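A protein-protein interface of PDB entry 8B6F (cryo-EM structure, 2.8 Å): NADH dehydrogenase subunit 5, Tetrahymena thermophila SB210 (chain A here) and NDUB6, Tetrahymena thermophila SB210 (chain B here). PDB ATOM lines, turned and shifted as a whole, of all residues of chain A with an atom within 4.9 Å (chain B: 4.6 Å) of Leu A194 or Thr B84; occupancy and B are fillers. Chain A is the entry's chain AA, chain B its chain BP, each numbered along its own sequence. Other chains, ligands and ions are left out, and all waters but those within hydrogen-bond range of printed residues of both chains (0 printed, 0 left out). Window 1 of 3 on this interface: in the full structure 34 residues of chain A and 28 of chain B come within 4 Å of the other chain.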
ATOM      1  N   SER A 187     -36.741 -14.316  19.708  1.00  0.00           N
ATOM      2  CA  SER A 187     -36.876 -13.062  20.435  1.00  0.00           C
ATOM      3  C   SER A 187     -38.028 -13.124  21.431  1.00  0.00           C
ATOM      4  O   SER A 187     -37.925 -12.586  22.539  1.00  0.00           O
ATOM      5  CB  SER A 187     -37.073 -11.913  19.449  1.00  0.00           C
ATOM      6  OG  SER A 187     -37.082 -10.667  20.119  1.00  0.00           O
ATOM      7  N   CYS A 190     -36.567 -15.387  24.342  1.00  0.00           N
ATOM      8  CA  CYS A 190     -35.505 -14.717  25.093  1.00  0.00           C
ATOM      9  C   CYS A 190     -35.770 -13.215  25.102  1.00  0.00           C
ATOM     10  O   CYS A 190     -35.163 -12.442  24.362  1.00  0.00           O
ATOM     11  CB  CYS A 190     -34.141 -15.030  24.485  1.00  0.00           C
ATOM     12  SG  CYS A 190     -33.845 -16.776  24.164  1.00  0.00           S
ATOM     13  N   LEU A 191     -36.690 -12.797  25.971  1.00  0.00           N
ATOM     14  CA  LEU A 191     -36.969 -11.373  26.111  1.00  0.00           C
ATOM     15  C   LEU A 191     -35.970 -10.695  27.039  1.00  0.00           C
ATOM     16  O   LEU A 191     -35.572  -9.551  26.797  1.00  0.00           O
ATOM     17  CB  LEU A 191     -38.394 -11.168  26.624  1.00  0.00           C
ATOM     18  CG  LEU A 191     -39.511 -11.430  25.613  1.00  0.00           C
ATOM     19  CD1 LEU A 191     -40.869 -11.426  26.294  1.00  0.00           C
ATOM     20  CD2 LEU A 191     -39.476 -10.401  24.498  1.00  0.00           C
ATOM     21  N   SER A 192     -35.554 -11.380  28.104  1.00  0.00           N
ATOM     22  CA  SER A 192     -34.621 -10.776  29.048  1.00  0.00           C
ATOM     23  C   SER A 192     -33.278 -10.491  28.394  1.00  0.00           C
ATOM     24  O   SER A 192     -32.664  -9.449  28.646  1.00  0.00           O
ATOM     25  CB  SER A 192     -34.438 -11.683  30.259  1.00  0.00           C
ATOM     26  OG  SER A 192     -35.641 -11.808  30.992  1.00  0.00           O
ATOM     27  N   TYR A 193     -32.798 -11.412  27.558  1.00  0.00           N
ATOM     28  CA  TYR A 193     -31.541 -11.179  26.856  1.00  0.00           C
ATOM     29  C   TYR A 193     -31.651  -9.975  25.934  1.00  0.00           C
ATOM     30  O   TYR A 193     -30.779  -9.098  25.929  1.00  0.00           O
ATOM     31  CB  TYR A 193     -31.151 -12.423  26.059  1.00  0.00           C
ATOM     32  CG  TYR A 193     -30.525 -13.515  26.889  1.00  0.00           C
ATOM     33  CD1 TYR A 193     -29.292 -13.329  27.495  1.00  0.00           C
ATOM     34  CD2 TYR A 193     -31.158 -14.737  27.051  1.00  0.00           C
ATOM     35  CE1 TYR A 193     -28.711 -14.325  28.245  1.00  0.00           C
ATOM     36  CE2 TYR A 193     -30.585 -15.740  27.799  1.00  0.00           C
ATOM     37  CZ  TYR A 193     -29.362 -15.527  28.395  1.00  0.00           C
ATOM     38  OH  TYR A 193     -28.784 -16.523  29.144  1.00  0.00           O
ATOM     39  N   LEU A 194     -32.719  -9.913  25.145  1.00  0.00           N
ATOM     40  CA  LEU A 194     -32.935  -8.828  24.193  1.00  0.00           C
ATOM     41  C   LEU A 194     -33.830  -7.793  24.860  1.00  0.00           C
ATOM     42  O   LEU A 194     -35.046  -7.973  24.952  1.00  0.00           O
ATOM     43  CB  LEU A 194     -33.566  -9.347  22.906  1.00  0.00           C
ATOM     44  CG  LEU A 194     -32.807 -10.430  22.145  1.00  0.00           C
ATOM     45  CD1 LEU A 194     -33.581 -10.818  20.902  1.00  0.00           C
ATOM     46  CD2 LEU A 194     -31.406  -9.968  21.788  1.00  0.00           C
ATOM     47  N   GLY A 195     -33.233  -6.698  25.313  1.00  0.00           N
ATOM     48  CA  GLY A 195     -34.011  -5.594  25.819  1.00  0.00           C
ATOM     49  C   GLY A 195     -34.845  -4.980  24.709  1.00  0.00           C
ATOM     50  O   GLY A 195     -35.023  -5.538  23.625  1.00  0.00           O
ATOM     51  N   LEU A 196     -35.382  -3.798  25.005  1.00  0.00           N
ATOM     52  CA  LEU A 196     -36.133  -3.064  23.995  1.00  0.00           C
ATOM     53  C   LEU A 196     -35.290  -2.860  22.742  1.00  0.00           C
ATOM     54  O   LEU A 196     -35.716  -3.185  21.629  1.00  0.00           O
ATOM     55  CB  LEU A 196     -36.593  -1.724  24.565  1.00  0.00           C
ATOM     56  CG  LEU A 196     -37.364  -0.807  23.617  1.00  0.00           C
ATOM     57  CD1 LEU A 196     -38.633  -1.479  23.119  1.00  0.00           C
ATOM     58  CD2 LEU A 196     -37.691   0.500  24.313  1.00  0.00           C
ATOM     59  N   GLY A 198     -32.460  -4.346  21.834  1.00  0.00           N
ATOM     60  CA  GLY A 198     -32.024  -5.591  21.225  1.00  0.00           C
ATOM     61  C   GLY A 198     -33.101  -6.218  20.365  1.00  0.00           C
ATOM     62  O   GLY A 198     -32.844  -6.641  19.236  1.00  0.00           O
ATOM     63  N   VAL A 199     -34.323  -6.296  20.888  1.00  0.00           N
ATOM     64  CA  VAL A 199     -35.424  -6.846  20.104  1.00  0.00           C
ATOM     65  C   VAL A 199     -35.644  -6.012  18.849  1.00  0.00           C
ATOM     66  O   VAL A 199     -35.795  -6.547  17.745  1.00  0.00           O
ATOM     67  CB  VAL A 199     -36.702  -6.927  20.960  1.00  0.00           C
ATOM     68  CG1 VAL A 199     -37.910  -7.287  20.105  1.00  0.00           C
ATOM     69  CG2 VAL A 199     -36.524  -7.940  22.075  1.00  0.00           C
ATOM     70  N   ILE A 201     -33.593  -4.050  17.139  1.00  0.00           N
ATOM     71  CA  ILE A 201     -32.532  -4.132  16.140  1.00  0.00           C
ATOM     72  C   ILE A 201     -32.505  -5.508  15.487  1.00  0.00           C
ATOM     73  O   ILE A 201     -32.363  -5.623  14.266  1.00  0.00           O
ATOM     74  CB  ILE A 201     -31.174  -3.779  16.774  1.00  0.00           C
ATOM     75  CG1 ILE A 201     -31.160  -2.322  17.251  1.00  0.00           C
ATOM     76  CG2 ILE A 201     -30.030  -4.027  15.789  1.00  0.00           C
ATOM     77  CD1 ILE A 201     -31.335  -1.287  16.152  1.00  0.00           C
ATOM     78  N   LEU A 202     -32.634  -6.572  16.283  1.00  0.00           N
ATOM     79  CA  LEU A 202     -32.610  -7.912  15.710  1.00  0.00           C
ATOM     80  C   LEU A 202     -33.731  -8.095  14.698  1.00  0.00           C
ATOM     81  O   LEU A 202     -33.496  -8.512  13.559  1.00  0.00           O
ATOM     82  CB  LEU A 202     -32.720  -8.952  16.825  1.00  0.00           C
ATOM     83  CG  LEU A 202     -32.713 -10.416  16.386  1.00  0.00           C
ATOM     84  CD1 LEU A 202     -31.441 -10.775  15.648  1.00  0.00           C
ATOM     85  CD2 LEU A 202     -32.911 -11.329  17.580  1.00  0.00           C
ATOM     86  N   TRP B  80     -27.245  -5.804  25.307  1.00  0.00           N
ATOM     87  CA  TRP B  80     -28.129  -6.138  24.196  1.00  0.00           C
ATOM     88  C   TRP B  80     -27.371  -6.246  22.880  1.00  0.00           C
ATOM     89  O   TRP B  80     -27.785  -6.994  21.989  1.00  0.00           O
ATOM     90  CB  TRP B  80     -29.254  -5.106  24.084  1.00  0.00           C
ATOM     91  CG  TRP B  80     -28.818  -3.732  23.672  1.00  0.00           C
ATOM     92  CD1 TRP B  80     -28.490  -2.695  24.496  1.00  0.00           C
ATOM     93  CD2 TRP B  80     -28.679  -3.239  22.333  1.00  0.00           C
ATOM     94  NE1 TRP B  80     -28.149  -1.590  23.753  1.00  0.00           N
ATOM     95  CE2 TRP B  80     -28.259  -1.899  22.423  1.00  0.00           C
ATOM     96  CE3 TRP B  80     -28.869  -3.804  21.069  1.00  0.00           C
ATOM     97  CZ2 TRP B  80     -28.020  -1.115  21.298  1.00  0.00           C
ATOM     98  CZ3 TRP B  80     -28.633  -3.025  19.951  1.00  0.00           C
ATOM     99  CH2 TRP B  80     -28.213  -1.694  20.072  1.00  0.00           C
ATOM    100  N   LYS B  81     -26.266  -5.512  22.730  1.00  0.00           N
ATOM    101  CA  LYS B  81     -25.497  -5.595  21.492  1.00  0.00           C
ATOM    102  C   LYS B  81     -24.934  -6.996  21.286  1.00  0.00           C
ATOM    103  O   LYS B  81     -25.128  -7.604  20.229  1.00  0.00           O
ATOM    104  CB  LYS B  81     -24.373  -4.561  21.500  1.00  0.00           C
ATOM    105  CG  LYS B  81     -24.863  -3.128  21.506  1.00  0.00           C
ATOM    106  CD  LYS B  81     -23.701  -2.153  21.502  1.00  0.00           C
ATOM    107  CE  LYS B  81     -24.183  -0.717  21.581  1.00  0.00           C
ATOM    108  NZ  LYS B  81     -24.951  -0.452  22.828  1.00  0.00           N
ATOM    109  N   TRP B  82     -24.231  -7.528  22.288  1.00  0.00           N
ATOM    110  CA  TRP B  82     -23.683  -8.874  22.157  1.00  0.00           C
ATOM    111  C   TRP B  82     -24.791  -9.917  22.111  1.00  0.00           C
ATOM    112  O   TRP B  82     -24.669 -10.928  21.410  1.00  0.00           O
ATOM    113  CB  TRP B  82     -22.718  -9.173  23.303  1.00  0.00           C
ATOM    114  CG  TRP B  82     -21.370  -8.554  23.125  1.00  0.00           C
ATOM    115  CD1 TRP B  82     -20.777  -7.636  23.938  1.00  0.00           C
ATOM    116  CD2 TRP B  82     -20.442  -8.811  22.065  1.00  0.00           C
ATOM    117  NE1 TRP B  82     -19.538  -7.305  23.451  1.00  0.00           N
ATOM    118  CE2 TRP B  82     -19.308  -8.012  22.301  1.00  0.00           C
ATOM    119  CE3 TRP B  82     -20.461  -9.640  20.938  1.00  0.00           C
ATOM    120  CZ2 TRP B  82     -18.203  -8.017  21.455  1.00  0.00           C
ATOM    121  CZ3 TRP B  82     -19.362  -9.642  20.097  1.00  0.00           C
ATOM    122  CH2 TRP B  82     -18.249  -8.836  20.359  1.00  0.00           C
ATOM    123  N   ASN B  83     -25.878  -9.693  22.849  1.00  0.00           N
ATOM    124  CA  ASN B  83     -27.001 -10.621  22.791  1.00  0.00           C
ATOM    125  C   ASN B  83     -27.568 -10.694  21.380  1.00  0.00           C
ATOM    126  O   ASN B  83     -27.844 -11.783  20.867  1.00  0.00           O
ATOM    127  CB  ASN B  83     -28.083 -10.207  23.788  1.00  0.00           C
ATOM    128  CG  ASN B  83     -27.601 -10.257  25.222  1.00  0.00           C
ATOM    129  OD1 ASN B  83     -26.623 -10.931  25.536  1.00  0.00           O
ATOM    130  ND2 ASN B  83     -28.297  -9.552  26.104  1.00  0.00           N
ATOM    131  N   THR B  84     -27.747  -9.540  20.734  1.00  0.00           N
ATOM    132  CA  THR B  84     -28.219  -9.538  19.355  1.00  0.00           C
ATOM    133  C   THR B  84     -27.218 -10.214  18.430  1.00  0.00           C
ATOM    134  O   THR B  84     -27.606 -10.965  17.527  1.00  0.00           O
ATOM    135  CB  THR B  84     -28.481  -8.105  18.892  1.00  0.00           C
ATOM    136  OG1 THR B  84     -29.410  -7.473  19.781  1.00  0.00           O
ATOM    137  CG2 THR B  84     -29.038  -8.090  17.477  1.00  0.00           C
ATOM    138  N   PHE B  85     -25.925  -9.964  18.637  1.00  0.00           N
ATOM    139  CA  PHE B  85     -24.913 -10.579  17.785  1.00  0.00           C
ATOM    140  C   PHE B  85     -24.966 -12.096  17.874  1.00  0.00           C
ATOM    141  O   PHE B  85     -24.884 -12.789  16.855  1.00  0.00           O
ATOM    142  CB  PHE B  85     -23.523 -10.073  18.169  1.00  0.00           C
ATOM    143  CG  PHE B  85     -22.426 -10.613  17.296  1.00  0.00           C
ATOM    144  CD1 PHE B  85     -21.838 -11.836  17.569  1.00  0.00           C
ATOM    145  CD2 PHE B  85     -21.985  -9.894  16.198  1.00  0.00           C
ATOM    146  CE1 PHE B  85     -20.832 -12.334  16.764  1.00  0.00           C
ATOM    147  CE2 PHE B  85     -20.979 -10.385  15.389  1.00  0.00           C
ATOM    148  CZ  PHE B  85     -20.402 -11.607  15.673  1.00  0.00           C
ATOM    149  N   HIS B  86     -25.107 -12.633  19.082  1.00  0.00           N
ATOM    150  CA  HIS B  86     -25.107 -14.072  19.286  1.00  0.00           C
ATOM    151  C   HIS B  86     -26.480 -14.699  19.101  1.00  0.00           C
ATOM    152  O   HIS B  86     -26.602 -15.922  19.208  1.00  0.00           O
ATOM    153  CB  HIS B  86     -24.570 -14.399  20.683  1.00  0.00           C
ATOM    154  CG  HIS B  86     -23.127 -14.046  20.868  1.00  0.00           C
ATOM    155  ND1 HIS B  86     -22.104 -14.772  20.296  1.00  0.00           N
ATOM    156  CD2 HIS B  86     -22.535 -13.038  21.551  1.00  0.00           C
ATOM    157  CE1 HIS B  86     -20.946 -14.228  20.622  1.00  0.00           C
ATOM    158  NE2 HIS B  86     -21.179 -13.176  21.382  1.00  0.00           N
ATOM    159  N   MET B  87     -27.517 -13.898  18.855  1.00  0.00           N
ATOM    160  CA  MET B  87     -28.820 -14.434  18.490  1.00  0.00           C
ATOM    161  C   MET B  87     -29.121 -14.328  17.002  1.00  0.00           C
ATOM    162  O   MET B  87     -29.997 -15.050  16.515  1.00  0.00           O
ATOM    163  CB  MET B  87     -29.929 -13.716  19.268  1.00  0.00           C
ATOM    164  CG  MET B  87     -29.967 -14.072  20.743  1.00  0.00           C
ATOM    165  SD  MET B  87     -31.410 -13.433  21.611  1.00  0.00           S
ATOM    166  CE  MET B  87     -32.745 -14.254  20.742  1.00  0.00           C
ATOM    167  N   PHE B  88     -28.427 -13.457  16.270  1.00  0.00           N
ATOM    168  CA  PHE B  88     -28.699 -13.276  14.849  1.00  0.00           C
ATOM    169  C   PHE B  88     -27.921 -14.270  13.990  1.00  0.00           C
ATOM    170  O   PHE B  88     -28.511 -15.027  13.213  1.00  0.00           O
ATOM    171  CB  PHE B  88     -28.368 -11.841  14.425  1.00  0.00           C
ATOM    172  CG  PHE B  88     -28.586 -11.583  12.965  1.00  0.00           C
ATOM    173  CD1 PHE B  88     -29.856 -11.323  12.479  1.00  0.00           C
ATOM    174  CD2 PHE B  88     -27.524 -11.604  12.078  1.00  0.00           C
ATOM    175  CE1 PHE B  88     -30.063 -11.088  11.134  1.00  0.00           C
ATOM    176  CE2 PHE B  88     -27.723 -11.369  10.733  1.00  0.00           C
ATOM    177  CZ  PHE B  88     -28.995 -11.109  10.260  1.00  0.00           C
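O of Tyr A193 sits at hydrogen-bond distance from ND2 of Asn B83 (2.5 Å).
O of Trp B80 sits at hydrogen-bond distance from OG1 of Thr B84 (2.8 Å).
CD2 of Leu A194 touches CB of Asn B83 (3.9 Å).
Thr B84 touches Leu A194.
CG of Leu A194 touches SD of Met B87 (3.4 Å).
CA of Gly A198 touches CE3 of Trp B80 (3.6 Å).
CA of Gly A198 touches OG1 of Thr B84, at 3.5 Å.
CZ3 of Trp B80 touches CG1 of Ile A201 (3.8 Å).
CG2 of Thr B84 touches CB of Leu A202, at 3.8 Å.
Leu A202 touches Phe B88.
Of the printed residues of chain B, Tyr A193 touches Asn B83 (2.5 Å).
Of chain B, only Asn B83, Thr B84 and Met B87 come within 4 Å of Leu A194.
Of the printed residues of chain B, Ile A201 touches Trp B80.
Thr B84 touches three residues of chain A.
Of the printed residues of chain A, Met B87 touches Leu A194.
Of the printed residues of chain A, Phe B88 touches Leu A202 (3.5 Å).
Hydrophobic or aromatic side chains of chain A that line the printed part of chain B: Leu A194, Ile A201 and Leu A202.
Of the 9 printed residues of chain B, 5 touch a printed residue of chain A.
Among the printed residues, 9 pairs touch across the chains.
Among the printed residues, no Asp or Glu carboxylate lies within 4 Å of a Lys or Arg side-chain nitrogen of the other chain.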
